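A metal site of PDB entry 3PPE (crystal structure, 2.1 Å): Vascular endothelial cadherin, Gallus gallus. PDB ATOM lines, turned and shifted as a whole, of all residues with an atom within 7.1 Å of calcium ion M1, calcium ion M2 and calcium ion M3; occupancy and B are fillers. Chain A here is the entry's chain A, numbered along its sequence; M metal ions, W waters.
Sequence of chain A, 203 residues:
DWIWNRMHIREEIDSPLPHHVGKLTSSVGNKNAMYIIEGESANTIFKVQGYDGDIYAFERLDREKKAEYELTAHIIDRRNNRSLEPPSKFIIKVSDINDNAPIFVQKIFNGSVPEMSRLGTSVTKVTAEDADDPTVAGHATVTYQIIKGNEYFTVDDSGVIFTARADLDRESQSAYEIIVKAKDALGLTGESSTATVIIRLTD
Within 4 Å of calcium ion M1: Glu 11, Glu 12, Asp 62, Glu 64 and Asp 99. The nearest printed residue that does not touch calcium ion M1 is Arg 63 (4.3 Å).
Calcium ion M1 is bound by OD1 of Asp 62, OE1 of Glu 64, OD2 of Asp 99, OE1 of Glu 11, water W1 and OE1 of Glu 12. Calcium ion M1 has six donor atoms within binding distance.
Seven residues have an atom within 4 Å of calcium ion M2: Glu 11, Glu 64, Asp 96, Ile 97, Asp 99, Asn 100 and Asp 132. Along chain A the residues within 4 Å of calcium ion M2 span positions 11 to 132.
Calcium ion M2 is bound by OD1 of Asp 99, OE2 of Glu 11, OD2 of Asp 96, O of Ile 97, OD1 of Asp 132, OE2 of Glu 64 and OE1 of Glu 64. Calcium ion M2 has seven donor atoms within binding distance.
The guanidinium group (NE) of Arg 63 lies close to the side-chain carboxylate (OD2) of Asp 96 (2.8 Å). N of Glu 12 lies within hydrogen-bond range of O of Leu 61, at 2.7 Å. OE1 of Glu 11 lies close to N of Arg 63 (2.9 Å). The backbone NH of Glu 11 lies within hydrogen-bond range of the backbone carbonyl oxygen of Ser 95 (3.1 Å). N of Asp 133 sits at hydrogen-bond distance from OD1 of Asp 96 (3.0 Å). OD2 of Asp 184 lies within hydrogen-bond range of N of Leu 188 (2.8 Å). N of Leu 186 lies close to OD2 of Asp 184 (3.0 Å). ND1 of His 139 is in hydrogen-bond range of OD1 of Asp 96 (2.8 Å).
Calcium ion M3 is bound by the backbone carbonyl oxygen (O) of His 139 (2.3 Å), the backbone carbonyl oxygen (O) of Asn 100 (2.3 Å), the side-chain carboxylate (OD2) of Asp 132 (2.4 Å), the side-chain amide oxygen (OD1) of Asn 98 (2.4 Å), the side-chain carboxylate (OD2) of Asp 130 (2.4 Å), the side-chain carboxylate (OD1) of Asp 130 (2.6 Å) and the side-chain carboxylate (OD1) of Asp 184 (2.6 Å). Calcium ion M3 has seven donor atoms within binding distance.
Within 4 Å of calcium ion M3: Asn 98, Asn 100, Asp 130, Asp 132, His 139 and Asp 184.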
ATOM      1  N   GLU A  11     -28.920   7.586 -30.836  1.00  0.00           N
ATOM      2  CA  GLU A  11     -28.018   7.055 -31.852  1.00  0.00           C
ATOM      3  C   GLU A  11     -28.798   6.467 -32.998  1.00  0.00           C
ATOM      4  O   GLU A  11     -29.977   6.120 -32.846  1.00  0.00           O
ATOM      5  CB  GLU A  11     -27.081   5.983 -31.264  1.00  0.00           C
ATOM      6  CG  GLU A  11     -27.857   4.767 -30.750  1.00  0.00           C
ATOM      7  CD  GLU A  11     -26.990   3.525 -30.552  1.00  0.00           C
ATOM      8  OE1 GLU A  11     -25.959   3.378 -31.252  1.00  0.00           O
ATOM      9  OE2 GLU A  11     -27.356   2.704 -29.691  1.00  0.00           O
ATOM     10  N   GLU A  12     -28.126   6.356 -34.149  1.00  0.00           N
ATOM     11  CA  GLU A  12     -28.629   5.582 -35.325  1.00  0.00           C
ATOM     12  C   GLU A  12     -29.941   6.143 -35.930  1.00  0.00           C
ATOM     13  O   GLU A  12     -30.775   5.406 -36.442  1.00  0.00           O
ATOM     14  CB  GLU A  12     -28.802   4.091 -34.971  1.00  0.00           C
ATOM     15  CG  GLU A  12     -27.612   3.446 -34.242  1.00  0.00           C
ATOM     16  CD  GLU A  12     -26.346   3.278 -35.067  1.00  0.00           C
ATOM     17  OE1 GLU A  12     -25.409   2.641 -34.548  1.00  0.00           O
ATOM     18  OE2 GLU A  12     -26.218   3.761 -36.215  1.00  0.00           O
ATOM     19  N   ARG A  60     -25.076  10.648 -38.590  1.00  0.00           N
ATOM     20  CA  ARG A  60     -25.692   9.631 -37.765  1.00  0.00           C
ATOM     21  C   ARG A  60     -24.653   9.163 -36.748  1.00  0.00           C
ATOM     22  O   ARG A  60     -23.456   9.036 -37.081  1.00  0.00           O
ATOM     23  CB  ARG A  60     -26.139   8.444 -38.604  1.00  0.00           C
ATOM     24  CG  ARG A  60     -27.337   8.741 -39.464  1.00  0.00           C
ATOM     25  CD  ARG A  60     -27.740   7.485 -40.216  1.00  0.00           C
ATOM     26  NE  ARG A  60     -27.956   6.391 -39.267  1.00  0.00           N
ATOM     27  CZ  ARG A  60     -27.143   5.351 -39.079  1.00  0.00           C
ATOM     28  NH1 ARG A  60     -26.021   5.196 -39.789  1.00  0.00           N
ATOM     29  NH2 ARG A  60     -27.472   4.445 -38.182  1.00  0.00           N
ATOM     30  N   LEU A  61     -25.101   8.914 -35.532  1.00  0.00           N
ATOM     31  CA  LEU A  61     -24.233   8.594 -34.424  1.00  0.00           C
ATOM     32  C   LEU A  61     -24.370   7.108 -33.955  1.00  0.00           C
ATOM     33  O   LEU A  61     -25.441   6.536 -33.979  1.00  0.00           O
ATOM     34  CB  LEU A  61     -24.545   9.538 -33.244  1.00  0.00           C
ATOM     35  CG  LEU A  61     -24.433  11.043 -33.539  1.00  0.00           C
ATOM     36  CD1 LEU A  61     -25.029  11.861 -32.393  1.00  0.00           C
ATOM     37  CD2 LEU A  61     -22.977  11.420 -33.850  1.00  0.00           C
ATOM     38  N   ASP A  62     -23.272   6.542 -33.503  1.00  0.00           N
ATOM     39  CA  ASP A  62     -23.294   5.191 -32.964  1.00  0.00           C
ATOM     40  C   ASP A  62     -22.787   5.283 -31.555  1.00  0.00           C
ATOM     41  O   ASP A  62     -21.618   5.529 -31.351  1.00  0.00           O
ATOM     42  CB  ASP A  62     -22.358   4.319 -33.811  1.00  0.00           C
ATOM     43  CG  ASP A  62     -22.316   2.871 -33.350  1.00  0.00           C
ATOM     44  OD1 ASP A  62     -23.056   2.456 -32.420  1.00  0.00           O
ATOM     45  OD2 ASP A  62     -21.507   2.148 -33.939  1.00  0.00           O
ATOM     46  N   ARG A  63     -23.675   5.100 -30.585  1.00  0.00           N
ATOM     47  CA  ARG A  63     -23.261   5.105 -29.157  1.00  0.00           C
ATOM     48  C   ARG A  63     -22.134   4.083 -28.864  1.00  0.00           C
ATOM     49  O   ARG A  63     -21.287   4.308 -27.997  1.00  0.00           O
ATOM     50  CB  ARG A  63     -24.468   4.870 -28.236  1.00  0.00           C
ATOM     51  CG  ARG A  63     -24.212   5.209 -26.776  1.00  0.00           C
ATOM     52  CD  ARG A  63     -25.118   4.346 -25.876  1.00  0.00           C
ATOM     53  NE  ARG A  63     -24.726   2.912 -25.977  1.00  0.00           N
ATOM     54  CZ  ARG A  63     -23.735   2.366 -25.270  1.00  0.00           C
ATOM     55  NH1 ARG A  63     -23.052   3.104 -24.426  1.00  0.00           N
ATOM     56  NH2 ARG A  63     -23.393   1.091 -25.444  1.00  0.00           N
ATOM     57  N   GLU A  64     -22.126   2.985 -29.599  1.00  0.00           N
ATOM     58  CA  GLU A  64     -21.111   1.959 -29.371  1.00  0.00           C
ATOM     59  C   GLU A  64     -19.720   2.348 -29.877  1.00  0.00           C
ATOM     60  O   GLU A  64     -18.723   1.724 -29.507  1.00  0.00           O
ATOM     61  CB  GLU A  64     -21.553   0.608 -29.962  1.00  0.00           C
ATOM     62  CG  GLU A  64     -22.592  -0.121 -29.102  1.00  0.00           C
ATOM     63  CD  GLU A  64     -23.976   0.481 -29.144  1.00  0.00           C
ATOM     64  OE1 GLU A  64     -24.555   0.693 -30.240  1.00  0.00           O
ATOM     65  OE2 GLU A  64     -24.530   0.733 -28.052  1.00  0.00           O
ATOM     66  N   LYS A  65     -19.648   3.396 -30.707  1.00  0.00           N
ATOM     67  CA  LYS A  65     -18.369   4.001 -31.123  1.00  0.00           C
ATOM     68  C   LYS A  65     -17.956   5.102 -30.132  1.00  0.00           C
ATOM     69  O   LYS A  65     -16.827   5.122 -29.637  1.00  0.00           O
ATOM     70  CB  LYS A  65     -18.602   4.676 -32.450  1.00  0.00           C
ATOM     71  CG  LYS A  65     -17.668   4.312 -33.558  1.00  0.00           C
ATOM     72  CD  LYS A  65     -18.040   2.940 -34.139  1.00  0.00           C
ATOM     73  CE  LYS A  65     -17.692   2.855 -35.629  1.00  0.00           C
ATOM     74  NZ  LYS A  65     -17.156   1.502 -35.973  1.00  0.00           N
ATOM     75  N   SER A  95     -27.947   8.708 -26.692  1.00  0.00           N
ATOM     76  CA  SER A  95     -28.910   7.818 -26.043  1.00  0.00           C
ATOM     77  C   SER A  95     -28.936   6.488 -26.784  1.00  0.00           C
ATOM     78  O   SER A  95     -29.029   6.454 -27.991  1.00  0.00           O
ATOM     79  CB  SER A  95     -30.324   8.423 -26.074  1.00  0.00           C
ATOM     80  OG  SER A  95     -30.278   9.745 -25.553  1.00  0.00           O
ATOM     81  N   ASP A  96     -28.873   5.404 -26.034  1.00  0.00           N
ATOM     82  CA  ASP A  96     -28.761   4.047 -26.562  1.00  0.00           C
ATOM     83  C   ASP A  96     -30.045   3.523 -27.200  1.00  0.00           C
ATOM     84  O   ASP A  96     -31.110   3.619 -26.607  1.00  0.00           O
ATOM     85  CB  ASP A  96     -28.390   3.107 -25.394  1.00  0.00           C
ATOM     86  CG  ASP A  96     -27.942   1.742 -25.862  1.00  0.00           C
ATOM     87  OD1 ASP A  96     -28.416   0.727 -25.285  1.00  0.00           O
ATOM     88  OD2 ASP A  96     -27.113   1.640 -26.798  1.00  0.00           O
ATOM     89  N   ILE A  97     -29.940   2.915 -28.366  1.00  0.00           N
ATOM     90  CA  ILE A  97     -31.002   2.041 -28.824  1.00  0.00           C
ATOM     91  C   ILE A  97     -30.514   0.590 -28.700  1.00  0.00           C
ATOM     92  O   ILE A  97     -29.302   0.318 -28.669  1.00  0.00           O
ATOM     93  CB  ILE A  97     -31.509   2.380 -30.285  1.00  0.00           C
ATOM     94  CG1 ILE A  97     -30.487   2.031 -31.380  1.00  0.00           C
ATOM     95  CG2 ILE A  97     -32.021   3.888 -30.374  1.00  0.00           C
ATOM     96  CD1 ILE A  97     -31.126   1.855 -32.795  1.00  0.00           C
ATOM     97  N   ASN A  98     -31.460  -0.335 -28.644  1.00  0.00           N
ATOM     98  CA  ASN A  98     -31.119  -1.746 -28.630  1.00  0.00           C
ATOM     99  C   ASN A  98     -30.760  -2.232 -30.043  1.00  0.00           C
ATOM    100  O   ASN A  98     -31.608  -2.670 -30.797  1.00  0.00           O
ATOM    101  CB  ASN A  98     -32.238  -2.593 -28.006  1.00  0.00           C
ATOM    102  CG  ASN A  98     -31.727  -3.974 -27.635  1.00  0.00           C
ATOM    103  OD1 ASN A  98     -30.583  -4.092 -27.134  1.00  0.00           O
ATOM    104  ND2 ASN A  98     -32.474  -5.005 -27.919  1.00  0.00           N
ATOM    105  N   ASP A  99     -29.499  -2.123 -30.416  1.00  0.00           N
ATOM    106  CA  ASP A  99     -29.101  -2.500 -31.756  1.00  0.00           C
ATOM    107  C   ASP A  99     -27.974  -3.547 -31.811  1.00  0.00           C
ATOM    108  O   ASP A  99     -27.414  -3.795 -32.855  1.00  0.00           O
ATOM    109  CB  ASP A  99     -28.787  -1.261 -32.621  1.00  0.00           C
ATOM    110  CG  ASP A  99     -27.677  -0.371 -32.063  1.00  0.00           C
ATOM    111  OD1 ASP A  99     -27.380  -0.361 -30.841  1.00  0.00           O
ATOM    112  OD2 ASP A  99     -27.082   0.394 -32.898  1.00  0.00           O
ATOM    113  N   ASN A 100     -27.657  -4.145 -30.653  1.00  0.00           N
ATOM    114  CA  ASN A 100     -26.691  -5.213 -30.572  1.00  0.00           C
ATOM    115  C   ASN A 100     -27.262  -6.445 -29.887  1.00  0.00           C
ATOM    116  O   ASN A 100     -28.023  -6.357 -28.905  1.00  0.00           O
ATOM    117  CB  ASN A 100     -25.384  -4.763 -29.861  1.00  0.00           C
ATOM    118  CG  ASN A 100     -24.655  -3.649 -30.612  1.00  0.00           C
ATOM    119  OD1 ASN A 100     -24.970  -2.474 -30.441  1.00  0.00           O
ATOM    120  ND2 ASN A 100     -23.728  -4.015 -31.484  1.00  0.00           N
ATOM    121  N   ALA A 101     -26.911  -7.605 -30.414  1.00  0.00           N
ATOM    122  CA  ALA A 101     -27.291  -8.862 -29.775  1.00  0.00           C
ATOM    123  C   ALA A 101     -26.101  -9.342 -28.903  1.00  0.00           C
ATOM    124  O   ALA A 101     -24.960  -8.896 -29.087  1.00  0.00           O
ATOM    125  CB  ALA A 101     -27.674  -9.910 -30.835  1.00  0.00           C
ATOM    126  N   PRO A 102     -26.372 -10.184 -27.894  1.00  0.00           N
ATOM    127  CA  PRO A 102     -25.219 -10.748 -27.142  1.00  0.00           C
ATOM    128  C   PRO A 102     -24.410 -11.672 -28.036  1.00  0.00           C
ATOM    129  O   PRO A 102     -24.987 -12.420 -28.884  1.00  0.00           O
ATOM    130  CB  PRO A 102     -25.890 -11.534 -25.995  1.00  0.00           C
ATOM    131  CG  PRO A 102     -27.339 -10.933 -25.952  1.00  0.00           C
ATOM    132  CD  PRO A 102     -27.662 -10.671 -27.387  1.00  0.00           C
ATOM    133  N   ASP A 130     -23.141  -8.171 -24.541  1.00  0.00           N
ATOM    134  CA  ASP A 130     -24.025  -7.387 -25.391  1.00  0.00           C
ATOM    135  C   ASP A 130     -23.483  -5.967 -25.325  1.00  0.00           C
ATOM    136  O   ASP A 130     -23.366  -5.413 -24.238  1.00  0.00           O
ATOM    137  CB  ASP A 130     -25.425  -7.435 -24.821  1.00  0.00           C
ATOM    138  CG  ASP A 130     -26.447  -6.783 -25.719  1.00  0.00           C
ATOM    139  OD1 ASP A 130     -26.317  -5.597 -26.113  1.00  0.00           O
ATOM    140  OD2 ASP A 130     -27.451  -7.441 -25.967  1.00  0.00           O
ATOM    141  N   ALA A 131     -23.185  -5.399 -26.501  1.00  0.00           N
ATOM    142  CA  ALA A 131     -22.499  -4.111 -26.606  1.00  0.00           C
ATOM    143  C   ALA A 131     -23.382  -2.879 -26.298  1.00  0.00           C
ATOM    144  O   ALA A 131     -22.886  -1.748 -26.215  1.00  0.00           O
ATOM    145  CB  ALA A 131     -21.909  -3.992 -27.993  1.00  0.00           C
ATOM    146  N   ASP A 132     -24.685  -3.082 -26.131  1.00  0.00           N
ATOM    147  CA  ASP A 132     -25.591  -1.994 -25.767  1.00  0.00           C
ATOM    148  C   ASP A 132     -25.325  -1.494 -24.342  1.00  0.00           C
ATOM    149  O   ASP A 132     -24.494  -2.059 -23.610  1.00  0.00           O
ATOM    150  CB  ASP A 132     -27.070  -2.367 -26.006  1.00  0.00           C
ATOM    151  CG  ASP A 132     -27.341  -2.613 -27.463  1.00  0.00           C
ATOM    152  OD1 ASP A 132     -26.916  -1.782 -28.267  1.00  0.00           O
ATOM    153  OD2 ASP A 132     -27.956  -3.654 -27.845  1.00  0.00           O
ATOM    154  N   ASP A 133     -26.035  -0.446 -23.961  1.00  0.00           N
ATOM    155  CA  ASP A 133     -25.799   0.214 -22.674  1.00  0.00           C
ATOM    156  C   ASP A 133     -26.467  -0.549 -21.533  1.00  0.00           C
ATOM    157  O   ASP A 133     -27.684  -0.734 -21.531  1.00  0.00           O
ATOM    158  CB  ASP A 133     -26.303   1.652 -22.712  1.00  0.00           C
ATOM    159  CG  ASP A 133     -25.881   2.449 -21.487  1.00  0.00           C
ATOM    160  OD1 ASP A 133     -25.929   3.690 -21.539  1.00  0.00           O
ATOM    161  OD2 ASP A 133     -25.508   1.826 -20.474  1.00  0.00           O
ATOM    162  N   GLY A 138     -32.771  -3.080 -20.086  1.00  0.00           N
ATOM    163  CA  GLY A 138     -32.783  -4.430 -20.600  1.00  0.00           C
ATOM    164  C   GLY A 138     -31.878  -4.592 -21.812  1.00  0.00           C
ATOM    165  O   GLY A 138     -31.701  -5.705 -22.319  1.00  0.00           O
ATOM    166  N   HIS A 139     -31.318  -3.488 -22.283  1.00  0.00           N
ATOM    167  CA  HIS A 139     -30.676  -3.450 -23.592  1.00  0.00           C
ATOM    168  C   HIS A 139     -29.486  -4.392 -23.651  1.00  0.00           C
ATOM    169  O   HIS A 139     -29.195  -4.968 -24.702  1.00  0.00           O
ATOM    170  CB  HIS A 139     -30.229  -2.019 -23.924  1.00  0.00           C
ATOM    171  CG  HIS A 139     -31.343  -1.133 -24.388  1.00  0.00           C
ATOM    172  ND1 HIS A 139     -31.124   0.062 -25.037  1.00  0.00           N
ATOM    173  CD2 HIS A 139     -32.697  -1.269 -24.303  1.00  0.00           C
ATOM    174  CE1 HIS A 139     -32.275   0.626 -25.327  1.00  0.00           C
ATOM    175  NE2 HIS A 139     -33.247  -0.160 -24.891  1.00  0.00           N
ATOM    176  N   ALA A 140     -28.799  -4.557 -22.522  1.00  0.00           N
ATOM    177  CA  ALA A 140     -27.638  -5.420 -22.453  1.00  0.00           C
ATOM    178  C   ALA A 140     -27.925  -6.549 -21.455  1.00  0.00           C
ATOM    179  O   ALA A 140     -27.001  -7.130 -20.865  1.00  0.00           O
ATOM    180  CB  ALA A 140     -26.462  -4.615 -22.023  1.00  0.00           C
ATOM    181  N   THR A 141     -29.185  -6.860 -21.251  1.00  0.00           N
ATOM    182  CA  THR A 141     -29.561  -7.943 -20.383  1.00  0.00           C
ATOM    183  C   THR A 141     -29.481  -9.242 -21.213  1.00  0.00           C
ATOM    184  O   THR A 141     -30.224  -9.391 -22.177  1.00  0.00           O
ATOM    185  CB  THR A 141     -31.012  -7.773 -19.891  1.00  0.00           C
ATOM    186  OG1 THR A 141     -31.124  -6.593 -19.088  1.00  0.00           O
ATOM    187  CG2 THR A 141     -31.422  -8.954 -19.010  1.00  0.00           C
ATOM    188  N   ASP A 184     -30.770 -11.038 -25.804  1.00  0.00           N
ATOM    189  CA  ASP A 184     -31.062  -9.978 -24.847  1.00  0.00           C
ATOM    190  C   ASP A 184     -32.557  -9.877 -24.579  1.00  0.00           C
ATOM    191  O   ASP A 184     -33.373 -10.391 -25.343  1.00  0.00           O
ATOM    192  CB  ASP A 184     -30.530  -8.635 -25.355  1.00  0.00           C
ATOM    193  CG  ASP A 184     -31.373  -8.053 -26.462  1.00  0.00           C
ATOM    194  OD1 ASP A 184     -30.888  -7.164 -27.191  1.00  0.00           O
ATOM    195  OD2 ASP A 184     -32.535  -8.491 -26.614  1.00  0.00           O
ATOM    196  N   ALA A 185     -32.914  -9.220 -23.477  1.00  0.00           N
ATOM    197  CA  ALA A 185     -34.238  -9.371 -22.891  1.00  0.00           C
ATOM    198  C   ALA A 185     -35.318  -8.811 -23.811  1.00  0.00           C
ATOM    199  O   ALA A 185     -36.502  -9.064 -23.621  1.00  0.00           O
ATOM    200  CB  ALA A 185     -34.298  -8.688 -21.534  1.00  0.00           C
ATOM    201  N   LEU A 186     -34.890  -8.050 -24.820  1.00  0.00           N
ATOM    202  CA  LEU A 186     -35.811  -7.486 -25.793  1.00  0.00           C
ATOM    203  C   LEU A 186     -35.920  -8.354 -27.032  1.00  0.00           C
ATOM    204  O   LEU A 186     -36.711  -8.083 -27.934  1.00  0.00           O
ATOM    205  CB  LEU A 186     -35.382  -6.066 -26.175  1.00  0.00           C
ATOM    206  CG  LEU A 186     -35.626  -4.973 -25.131  1.00  0.00           C
ATOM    207  CD1 LEU A 186     -34.568  -5.034 -24.047  1.00  0.00           C
ATOM    208  CD2 LEU A 186     -35.649  -3.596 -25.791  1.00  0.00           C
ATOM    209  N   LEU A 188     -33.291  -9.664 -29.014  1.00  0.00           N
ATOM    210  CA  LEU A 188     -32.308  -9.499 -30.084  1.00  0.00           C
ATOM    211  C   LEU A 188     -31.346 -10.676 -30.134  1.00  0.00           C
ATOM    212  O   LEU A 188     -30.566 -10.893 -29.215  1.00  0.00           O
ATOM    213  CB  LEU A 188     -31.536  -8.193 -29.892  1.00  0.00           C
ATOM    214  CG  LEU A 188     -31.374  -7.310 -31.139  1.00  0.00           C
ATOM    215  CD1 LEU A 188     -32.721  -7.095 -31.822  1.00  0.00           C
ATOM    216  CD2 LEU A 188     -30.728  -5.981 -30.781  1.00  0.00           C
HETATM  217 CA    CA M   1     -25.102   1.478 -32.344  1.00  0.00          CA
HETATM  218 CA    CA M   2     -26.916   0.574 -28.862  1.00  0.00          CA
HETATM  219 CA    CA M   3     -28.791  -5.629 -26.857  1.00  0.00          CA
HETATM  220  O   HOH W   1     -24.206  -0.705 -33.070  1.00  0.00           O
